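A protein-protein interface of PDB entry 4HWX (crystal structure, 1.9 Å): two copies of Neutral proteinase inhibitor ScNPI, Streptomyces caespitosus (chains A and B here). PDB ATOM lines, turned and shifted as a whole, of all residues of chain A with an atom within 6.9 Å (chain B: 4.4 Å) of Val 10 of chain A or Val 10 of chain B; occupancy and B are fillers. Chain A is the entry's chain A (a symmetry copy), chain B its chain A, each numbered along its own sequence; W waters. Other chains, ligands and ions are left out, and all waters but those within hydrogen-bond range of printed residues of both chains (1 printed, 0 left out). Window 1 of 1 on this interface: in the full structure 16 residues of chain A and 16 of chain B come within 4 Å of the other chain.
Of the 10 printed residues of chain B, 5 touch a printed residue of chain A.
Along chain B the printed residues that touch a printed residue of chain A span positions 8 to 83.
Of the 19 printed residues of chain A, 7 touch a printed residue of chain B.
Hydrophobic or aromatic side chains of chain A within 4 Å of the printed part of chain B: Ala 8, Val 10 and Ala 27.
Water W1 lies within hydrogen-bond range of the guanidinium group of Arg 89 of chain A (2.6 Å), the side-chain carboxylate of Asp 82 of chain B (2.7 Å), the side-chain hydroxyl of Thr 80 of chain B (2.7 Å) and the backbone carbonyl oxygen of Val 10 of chain B (2.9 Å).
Ala 8 of chain A touches Val 10 of chain B, and with the chains exchanged Val 10 of chain A touches Ala 8 of chain B.
Val 10 of chain A touches its own counterpart, Val 10 of chain B.
Val 10 of chain A touches Gly 83 of chain B, and with the chains exchanged Gly 83 of chain A touches Val 10 of chain B.
Asp 82 of chain A touches its own counterpart, Asp 82 of chain B.
10 positions are printed for both chains.
Of the 12 pairs that touch across the chains among the printed residues, 8 have their exchanged pair printed and touching as well.
Printed residues of chain B within 4 Å of Ala 8 of chain A: Val 10 (3.4 Å).
Printed residues of chain B within 4 Å of Ala 27 of chain A: Ala 8 (3.9 Å).
Printed residues of chain B within 4 Å of Thr 29 of chain A: Ala 8.
Ala 81 of chain A touches none of the printed residues of chain B.
Printed residues of chain B within 4 Å of Gly 83 of chain A: Val 10 (3.7 Å).
Of the printed residues of chain A, Gly 83 of chain B touches Val 10 (3.7 Å).
The nearest printed residue of chain B that does not touch Val 10 of chain A is Met 9 of chain B (4.4 Å).
The nearest residue of chain A that does not touch Val 10 of chain B is Met 9 of chain A (4.4 Å).
Val 10 of chain B touches Ala 8 of chain A (CG2 to O, 3.4 Å).
Val 10 of chain A touches Ala 8 of chain B (CG2 to O, 3.4 Å).
CG1 of Val 10 of chain A touches CG1 of Val 10 of chain B, at 3.7 Å.
Val 10 of chain A touches Asp 82 of chain B.
Gly 83 of chain B touches Val 10 of chain A (CA to CG1, 3.7 Å).
Thr 29 of chain A touches Ala 8 of chain B.
Val 10 of chain B touches Asp 82 of chain A (CG1 to O, 3.5 Å).
Asp 82 of chain A touches Asp 82 of chain B (CB to CB, 3.8 Å).
Val 10 of chain B touches Gly 83 of chain A.
Thr 80 of chain B touches Arg 89 of chain A.
The side-chain carboxylate (OD2) of Asp 82 of chain B lies within salt-bridge range of the guanidinium group (NH2) of Arg 89 of chain A, at 2.8 Å.
The backbone NH (N) of Val 10 of chain A lies within hydrogen-bond range of the backbone carbonyl oxygen (O) of Asp 82 of chain A.
O of Ala 8 of chain A sits at hydrogen-bond distance from N of Val 84 of chain A.
The backbone carbonyl oxygen (O) of Gly 83 of chain A lies within hydrogen-bond range of the guanidinium group (NE) of Arg 89 of chain A, 3.2 Å away.
The backbone NH (N) of Val 10 of chain B sits at hydrogen-bond distance from the backbone carbonyl oxygen (O) of Asp 82 of chain B, at 2.9 Å.
O of Gly 83 of chain A sits at hydrogen-bond distance from N of Val 90 of chain A (2.9 Å).
OG1 of Thr 12 of chain B sits at hydrogen-bond distance from OG1 of Thr 80 of chain B, 2.7 Å away.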
ATOM      1  N   SER A   7      10.877 -33.993   3.678  1.00  0.00           N
ATOM      2  CA  SER A   7      11.797 -34.193   2.559  1.00  0.00           C
ATOM      3  C   SER A   7      11.034 -33.983   1.273  1.00  0.00           C
ATOM      4  O   SER A   7      10.248 -34.841   0.855  1.00  0.00           O
ATOM      5  CB  SER A   7      12.443 -35.576   2.620  1.00  0.00           C
ATOM      6  OG  SER A   7      13.301 -35.684   3.742  1.00  0.00           O
ATOM      7  N   ALA A   8      11.234 -32.803   0.675  1.00  0.00           N
ATOM      8  CA  ALA A   8      10.597 -32.353  -0.559  1.00  0.00           C
ATOM      9  C   ALA A   8      11.610 -31.549  -1.363  1.00  0.00           C
ATOM     10  O   ALA A   8      12.159 -30.561  -0.880  1.00  0.00           O
ATOM     11  CB  ALA A   8       9.355 -31.520  -0.238  1.00  0.00           C
ATOM     12  N   MET A   9      11.887 -32.001  -2.580  1.00  0.00           N
ATOM     13  CA  MET A   9      12.928 -31.418  -3.409  1.00  0.00           C
ATOM     14  C   MET A   9      12.511 -31.211  -4.841  1.00  0.00           C
ATOM     15  O   MET A   9      11.640 -31.910  -5.361  1.00  0.00           O
ATOM     16  CB  MET A   9      14.155 -32.383  -3.428  1.00  0.00           C
ATOM     17  CG  MET A   9      14.813 -32.641  -2.047  1.00  0.00           C
ATOM     18  SD  MET A   9      15.672 -31.179  -1.417  1.00  0.00           S
ATOM     19  CE  MET A   9      16.990 -31.046  -2.624  1.00  0.00           C
ATOM     20  N   VAL A  10      13.236 -30.329  -5.511  1.00  0.00           N
ATOM     21  CA  VAL A  10      13.132 -30.118  -6.949  1.00  0.00           C
ATOM     22  C   VAL A  10      14.566 -30.177  -7.495  1.00  0.00           C
ATOM     23  O   VAL A  10      15.479 -29.564  -6.924  1.00  0.00           O
ATOM     24  CB  VAL A  10      12.362 -28.834  -7.378  1.00  0.00           C
ATOM     25  CG1 VAL A  10      12.971 -27.588  -6.748  1.00  0.00           C
ATOM     26  CG2 VAL A  10      12.346 -28.690  -8.909  1.00  0.00           C
ATOM     27  N   PHE A  11      14.761 -30.957  -8.558  1.00  0.00           N
ATOM     28  CA  PHE A  11      16.042 -31.085  -9.247  1.00  0.00           C
ATOM     29  C   PHE A  11      15.927 -30.539 -10.653  1.00  0.00           C
ATOM     30  O   PHE A  11      14.939 -30.811 -11.321  1.00  0.00           O
ATOM     31  CB  PHE A  11      16.502 -32.552  -9.295  1.00  0.00           C
ATOM     32  CG  PHE A  11      16.548 -33.177  -7.921  1.00  0.00           C
ATOM     33  CD1 PHE A  11      17.587 -32.885  -7.044  1.00  0.00           C
ATOM     34  CD2 PHE A  11      15.527 -34.019  -7.488  1.00  0.00           C
ATOM     35  CE1 PHE A  11      17.601 -33.418  -5.755  1.00  0.00           C
ATOM     36  CE2 PHE A  11      15.547 -34.563  -6.200  1.00  0.00           C
ATOM     37  CZ  PHE A  11      16.600 -34.281  -5.356  1.00  0.00           C
ATOM     38  N   THR A  12      16.898 -29.748 -11.102  1.00  0.00           N
ATOM     39  CA  THR A  12      16.854 -29.224 -12.470  1.00  0.00           C
ATOM     40  C   THR A  12      18.221 -29.406 -13.145  1.00  0.00           C
ATOM     41  O   THR A  12      19.258 -29.580 -12.485  1.00  0.00           O
ATOM     42  CB  THR A  12      16.386 -27.746 -12.575  1.00  0.00           C
ATOM     43  OG1 THR A  12      17.481 -26.841 -12.455  1.00  0.00           O
ATOM     44  CG2 THR A  12      15.216 -27.381 -11.638  1.00  0.00           C
ATOM     45  N   ALA A  27      13.429 -30.889 -15.444  1.00  0.00           N
ATOM     46  CA  ALA A  27      13.285 -30.853 -13.997  1.00  0.00           C
ATOM     47  C   ALA A  27      12.395 -31.959 -13.481  1.00  0.00           C
ATOM     48  O   ALA A  27      11.502 -32.411 -14.206  1.00  0.00           O
ATOM     49  CB  ALA A  27      12.699 -29.509 -13.569  1.00  0.00           C
ATOM     50  N   THR A  28      12.606 -32.358 -12.196  1.00  0.00           N
ATOM     51  CA  THR A  28      11.738 -33.316 -11.507  1.00  0.00           C
ATOM     52  C   THR A  28      11.447 -32.886 -10.071  1.00  0.00           C
ATOM     53  O   THR A  28      12.242 -32.168  -9.456  1.00  0.00           O
ATOM     54  CB  THR A  28      12.313 -34.744 -11.470  1.00  0.00           C
ATOM     55  OG1 THR A  28      13.599 -34.723 -10.858  1.00  0.00           O
ATOM     56  CG2 THR A  28      12.354 -35.416 -12.839  1.00  0.00           C
ATOM     57  N   THR A  29      10.313 -33.350  -9.539  1.00  0.00           N
ATOM     58  CA  THR A  29       9.944 -33.172  -8.135  1.00  0.00           C
ATOM     59  C   THR A  29      10.188 -34.500  -7.422  1.00  0.00           C
ATOM     60  O   THR A  29      10.142 -35.565  -8.054  1.00  0.00           O
ATOM     61  CB  THR A  29       8.490 -32.747  -7.946  1.00  0.00           C
ATOM     62  OG1 THR A  29       7.653 -33.795  -8.456  1.00  0.00           O
ATOM     63  CG2 THR A  29       8.168 -31.364  -8.560  1.00  0.00           C
ATOM     64  N   LEU A  30      10.398 -34.438  -6.118  1.00  0.00           N
ATOM     65  CA  LEU A  30      10.616 -35.620  -5.289  1.00  0.00           C
ATOM     66  C   LEU A  30      10.193 -35.363  -3.852  1.00  0.00           C
ATOM     67  O   LEU A  30      10.549 -34.345  -3.247  1.00  0.00           O
ATOM     68  CB  LEU A  30      12.083 -36.065  -5.330  1.00  0.00           C
ATOM     69  CG  LEU A  30      12.396 -37.373  -4.578  1.00  0.00           C
ATOM     70  CD1 LEU A  30      11.807 -38.571  -5.289  1.00  0.00           C
ATOM     71  CD2 LEU A  30      13.891 -37.564  -4.400  1.00  0.00           C
ATOM     72  N   THR A  80      20.974 -28.548 -10.288  1.00  0.00           N
ATOM     73  CA  THR A  80      20.513 -27.836  -9.089  1.00  0.00           C
ATOM     74  C   THR A  80      19.678 -28.767  -8.237  1.00  0.00           C
ATOM     75  O   THR A  80      19.061 -29.696  -8.756  1.00  0.00           O
ATOM     76  CB  THR A  80      19.709 -26.557  -9.416  1.00  0.00           C
ATOM     77  OG1 THR A  80      18.446 -26.907  -9.983  1.00  0.00           O
ATOM     78  CG2 THR A  80      20.458 -25.576 -10.297  1.00  0.00           C
ATOM     79  N   ALA A  81      19.699 -28.543  -6.922  1.00  0.00           N
ATOM     80  CA  ALA A  81      18.899 -29.280  -5.953  1.00  0.00           C
ATOM     81  C   ALA A  81      18.412 -28.277  -4.910  1.00  0.00           C
ATOM     82  O   ALA A  81      19.227 -27.553  -4.335  1.00  0.00           O
ATOM     83  CB  ALA A  81      19.721 -30.392  -5.324  1.00  0.00           C
ATOM     84  N   ASP A  82      17.089 -28.110  -4.789  1.00  0.00           N
ATOM     85  CA  ASP A  82      16.521 -27.158  -3.818  1.00  0.00           C
ATOM     86  C   ASP A  82      15.336 -27.761  -3.109  1.00  0.00           C
ATOM     87  O   ASP A  82      14.573 -28.499  -3.728  1.00  0.00           O
ATOM     88  CB  ASP A  82      16.088 -25.835  -4.484  1.00  0.00           C
ATOM     89  CG  ASP A  82      17.199 -25.064  -5.158  1.00  0.00           C
ATOM     90  OD1 ASP A  82      17.811 -24.213  -4.497  1.00  0.00           O
ATOM     91  OD2 ASP A  82      17.412 -25.269  -6.376  1.00  0.00           O
ATOM     92  N   GLY A  83      15.163 -27.394  -1.837  1.00  0.00           N
ATOM     93  CA  GLY A  83      14.018 -27.828  -1.052  1.00  0.00           C
ATOM     94  C   GLY A  83      14.368 -28.108   0.376  1.00  0.00           C
ATOM     95  O   GLY A  83      15.055 -27.302   1.015  1.00  0.00           O
ATOM     96  N   VAL A  84      13.905 -29.252   0.879  1.00  0.00           N
ATOM     97  CA  VAL A  84      14.191 -29.648   2.259  1.00  0.00           C
ATOM     98  C   VAL A  84      14.493 -31.139   2.260  1.00  0.00           C
ATOM     99  O   VAL A  84      13.874 -31.881   1.514  1.00  0.00           O
ATOM    100  CB  VAL A  84      13.042 -29.229   3.238  1.00  0.00           C
ATOM    101  CG1 VAL A  84      11.689 -29.816   2.847  1.00  0.00           C
ATOM    102  CG2 VAL A  84      13.380 -29.566   4.681  1.00  0.00           C
ATOM    103  N   ARG A  89      16.961 -27.290   5.093  1.00  0.00           N
ATOM    104  CA  ARG A  89      16.853 -26.543   3.841  1.00  0.00           C
ATOM    105  C   ARG A  89      18.075 -26.876   2.975  1.00  0.00           C
ATOM    106  O   ARG A  89      19.200 -26.934   3.483  1.00  0.00           O
ATOM    107  CB  ARG A  89      16.745 -25.031   4.151  1.00  0.00           C
ATOM    108  CG  ARG A  89      16.369 -24.151   2.953  1.00  0.00           C
ATOM    109  CD  ARG A  89      14.898 -23.739   2.933  1.00  0.00           C
ATOM    110  NE  ARG A  89      14.200 -24.329   1.789  1.00  0.00           N
ATOM    111  CZ  ARG A  89      14.146 -23.795   0.572  1.00  0.00           C
ATOM    112  NH1 ARG A  89      14.704 -22.614   0.327  1.00  0.00           N
ATOM    113  NH2 ARG A  89      13.517 -24.429  -0.409  1.00  0.00           N
ATOM    114  N   VAL A  90      17.835 -27.166   1.690  1.00  0.00           N
ATOM    115  CA  VAL A  90      18.861 -27.535   0.711  1.00  0.00           C
ATOM    116  C   VAL A  90      18.797 -26.539  -0.461  1.00  0.00           C
ATOM    117  O   VAL A  90      17.726 -26.286  -0.970  1.00  0.00           O
ATOM    118  CB  VAL A  90      18.684 -29.013   0.219  1.00  0.00           C
ATOM    119  CG1 VAL A  90      19.616 -29.339  -0.962  1.00  0.00           C
ATOM    120  CG2 VAL A  90      18.890 -30.014   1.363  1.00  0.00           C
ATOM    121  N   TYR A 112      19.912 -37.777 -10.535  1.00  0.00           N
ATOM    122  CA  TYR A 112      19.888 -37.096 -11.830  1.00  0.00           C
ATOM    123  C   TYR A 112      19.639 -38.055 -13.008  1.00  0.00           C
ATOM    124  O   TYR A 112      19.940 -37.706 -14.152  1.00  0.00           O
ATOM    125  CB  TYR A 112      21.150 -36.246 -12.039  1.00  0.00           C
ATOM    126  CG  TYR A 112      21.112 -35.025 -11.145  1.00  0.00           C
ATOM    127  CD1 TYR A 112      20.282 -33.941 -11.448  1.00  0.00           C
ATOM    128  CD2 TYR A 112      21.761 -35.020  -9.909  1.00  0.00           C
ATOM    129  CE1 TYR A 112      20.149 -32.859 -10.572  1.00  0.00           C
ATOM    130  CE2 TYR A 112      21.673 -33.921  -9.049  1.00  0.00           C
ATOM    131  CZ  TYR A 112      20.869 -32.843  -9.386  1.00  0.00           C
ATOM    132  OH  TYR A 112      20.759 -31.769  -8.530  1.00  0.00           O
ATOM    133  N   PHE A 114      17.189 -38.602 -15.047  1.00  0.00           N
ATOM    134  CA  PHE A 114      15.966 -38.062 -15.672  1.00  0.00           C
ATOM    135  C   PHE A 114      16.312 -37.157 -16.864  1.00  0.00           C
ATOM    136  O   PHE A 114      17.458 -36.669 -16.917  1.00  0.00           O
ATOM    137  CB  PHE A 114      15.090 -37.306 -14.645  1.00  0.00           C
ATOM    138  CG  PHE A 114      15.667 -36.031 -14.070  1.00  0.00           C
ATOM    139  CD1 PHE A 114      15.427 -34.803 -14.677  1.00  0.00           C
ATOM    140  CD2 PHE A 114      16.386 -36.051 -12.877  1.00  0.00           C
ATOM    141  CE1 PHE A 114      15.940 -33.620 -14.132  1.00  0.00           C
ATOM    142  CE2 PHE A 114      16.898 -34.865 -12.328  1.00  0.00           C
ATOM    143  CZ  PHE A 114      16.672 -33.657 -12.956  1.00  0.00           C
ATOM    144  OXT PHE A 114      15.414 -36.889 -17.702  1.00  0.00           O
ATOM    145  N   ALA B   8       8.231 -27.072 -12.139  1.00  0.00           N
ATOM    146  CA  ALA B   8       8.460 -27.966 -11.007  1.00  0.00           C
ATOM    147  C   ALA B   8       8.948 -27.140  -9.826  1.00  0.00           C
ATOM    148  O   ALA B   8       9.953 -26.438  -9.918  1.00  0.00           O
ATOM    149  CB  ALA B   8       9.473 -29.047 -11.387  1.00  0.00           C
ATOM    150  N   MET B   9       8.207 -27.191  -8.726  1.00  0.00           N
ATOM    151  CA  MET B   9       8.471 -26.355  -7.568  1.00  0.00           C
ATOM    152  C   MET B   9       8.397 -27.096  -6.260  1.00  0.00           C
ATOM    153  O   MET B   9       7.698 -28.104  -6.135  1.00  0.00           O
ATOM    154  CB  MET B   9       7.399 -25.222  -7.510  1.00  0.00           C
ATOM    155  CG  MET B   9       7.388 -24.262  -8.728  1.00  0.00           C
ATOM    156  SD  MET B   9       8.852 -23.200  -8.774  1.00  0.00           S
ATOM    157  CE  MET B   9       8.566 -22.210  -7.307  1.00  0.00           C
ATOM    158  N   VAL B  10       9.021 -26.512  -5.250  1.00  0.00           N
ATOM    159  CA  VAL B  10       8.915 -26.952  -3.865  1.00  0.00           C
ATOM    160  C   VAL B  10       8.579 -25.699  -3.043  1.00  0.00           C
ATOM    161  O   VAL B  10       9.202 -24.644  -3.227  1.00  0.00           O
ATOM    162  CB  VAL B  10      10.146 -27.735  -3.321  1.00  0.00           C
ATOM    163  CG1 VAL B  10      11.427 -26.926  -3.474  1.00  0.00           C
ATOM    164  CG2 VAL B  10       9.944 -28.116  -1.845  1.00  0.00           C
ATOM    165  N   PHE B  11       7.565 -25.810  -2.186  1.00  0.00           N
ATOM    166  CA  PHE B  11       7.146 -24.744  -1.279  1.00  0.00           C
ATOM    167  C   PHE B  11       7.372 -25.171   0.154  1.00  0.00           C
ATOM    168  O   PHE B  11       7.067 -26.304   0.496  1.00  0.00           O
ATOM    169  CB  PHE B  11       5.665 -24.388  -1.490  1.00  0.00           C
ATOM    170  CG  PHE B  11       5.363 -24.041  -2.927  1.00  0.00           C
ATOM    171  CD1 PHE B  11       5.729 -22.806  -3.451  1.00  0.00           C
ATOM    172  CD2 PHE B  11       4.755 -24.968  -3.770  1.00  0.00           C
ATOM    173  CE1 PHE B  11       5.500 -22.505  -4.794  1.00  0.00           C
ATOM    174  CE2 PHE B  11       4.515 -24.664  -5.114  1.00  0.00           C
ATOM    175  CZ  PHE B  11       4.864 -23.423  -5.606  1.00  0.00           C
ATOM    176  N   THR B  12       7.931 -24.297   0.988  1.00  0.00           N
ATOM    177  CA  THR B  12       8.137 -24.646   2.397  1.00  0.00           C
ATOM    178  C   THR B  12       7.660 -23.496   3.296  1.00  0.00           C
ATOM    179  O   THR B  12       7.527 -22.340   2.864  1.00  0.00           O
ATOM    180  CB  THR B  12       9.596 -25.048   2.751  1.00  0.00           C
ATOM    181  OG1 THR B  12      10.380 -23.910   3.104  1.00  0.00           O
ATOM    182  CG2 THR B  12      10.287 -25.933   1.694  1.00  0.00           C
ATOM    183  N   THR B  28       5.626 -28.858   0.422  1.00  0.00           N
ATOM    184  CA  THR B  28       4.948 -29.581  -0.657  1.00  0.00           C
ATOM    185  C   THR B  28       5.718 -29.490  -1.972  1.00  0.00           C
ATOM    186  O   THR B  28       6.465 -28.533  -2.199  1.00  0.00           O
ATOM    187  CB  THR B  28       3.510 -29.089  -0.910  1.00  0.00           C
ATOM    188  OG1 THR B  28       3.528 -27.694  -1.194  1.00  0.00           O
ATOM    189  CG2 THR B  28       2.548 -29.419   0.226  1.00  0.00           C
ATOM    190  N   THR B  80       8.832 -20.089   1.426  1.00  0.00           N
ATOM    191  CA  THR B  80       9.840 -20.206   0.366  1.00  0.00           C
ATOM    192  C   THR B  80       9.221 -20.855  -0.852  1.00  0.00           C
ATOM    193  O   THR B  80       8.272 -21.628  -0.727  1.00  0.00           O
ATOM    194  CB  THR B  80      11.094 -20.997   0.806  1.00  0.00           C
ATOM    195  OG1 THR B  80      10.765 -22.377   0.971  1.00  0.00           O
ATOM    196  CG2 THR B  80      11.764 -20.435   2.044  1.00  0.00           C
ATOM    197  N   ALA B  81       9.730 -20.503  -2.034  1.00  0.00           N
ATOM    198  CA  ALA B  81       9.321 -21.080  -3.307  1.00  0.00           C
ATOM    199  C   ALA B  81      10.580 -21.245  -4.156  1.00  0.00           C
ATOM    200  O   ALA B  81      11.321 -20.278  -4.339  1.00  0.00           O
ATOM    201  CB  ALA B  81       8.297 -20.189  -3.988  1.00  0.00           C
ATOM    202  N   ASP B  82      10.913 -22.488  -4.527  1.00  0.00           N
ATOM    203  CA  ASP B  82      12.114 -22.752  -5.338  1.00  0.00           C
ATOM    204  C   ASP B  82      11.819 -23.757  -6.420  1.00  0.00           C
ATOM    205  O   ASP B  82      11.049 -24.686  -6.187  1.00  0.00           O
ATOM    206  CB  ASP B  82      13.294 -23.263  -4.485  1.00  0.00           C
ATOM    207  CG  ASP B  82      13.768 -22.311  -3.411  1.00  0.00           C
ATOM    208  OD1 ASP B  82      14.673 -21.513  -3.690  1.00  0.00           O
ATOM    209  OD2 ASP B  82      13.274 -22.413  -2.265  1.00  0.00           O
ATOM    210  N   GLY B  83      12.478 -23.596  -7.569  1.00  0.00           N
ATOM    211  CA  GLY B  83      12.359 -24.537  -8.673  1.00  0.00           C
ATOM    212  C   GLY B  83      12.370 -23.864 -10.010  1.00  0.00           C
ATOM    213  O   GLY B  83      13.218 -23.002 -10.262  1.00  0.00           O
HETATM  214  O   HOH W   1      11.167 -23.741  -1.338  1.00  0.00           O
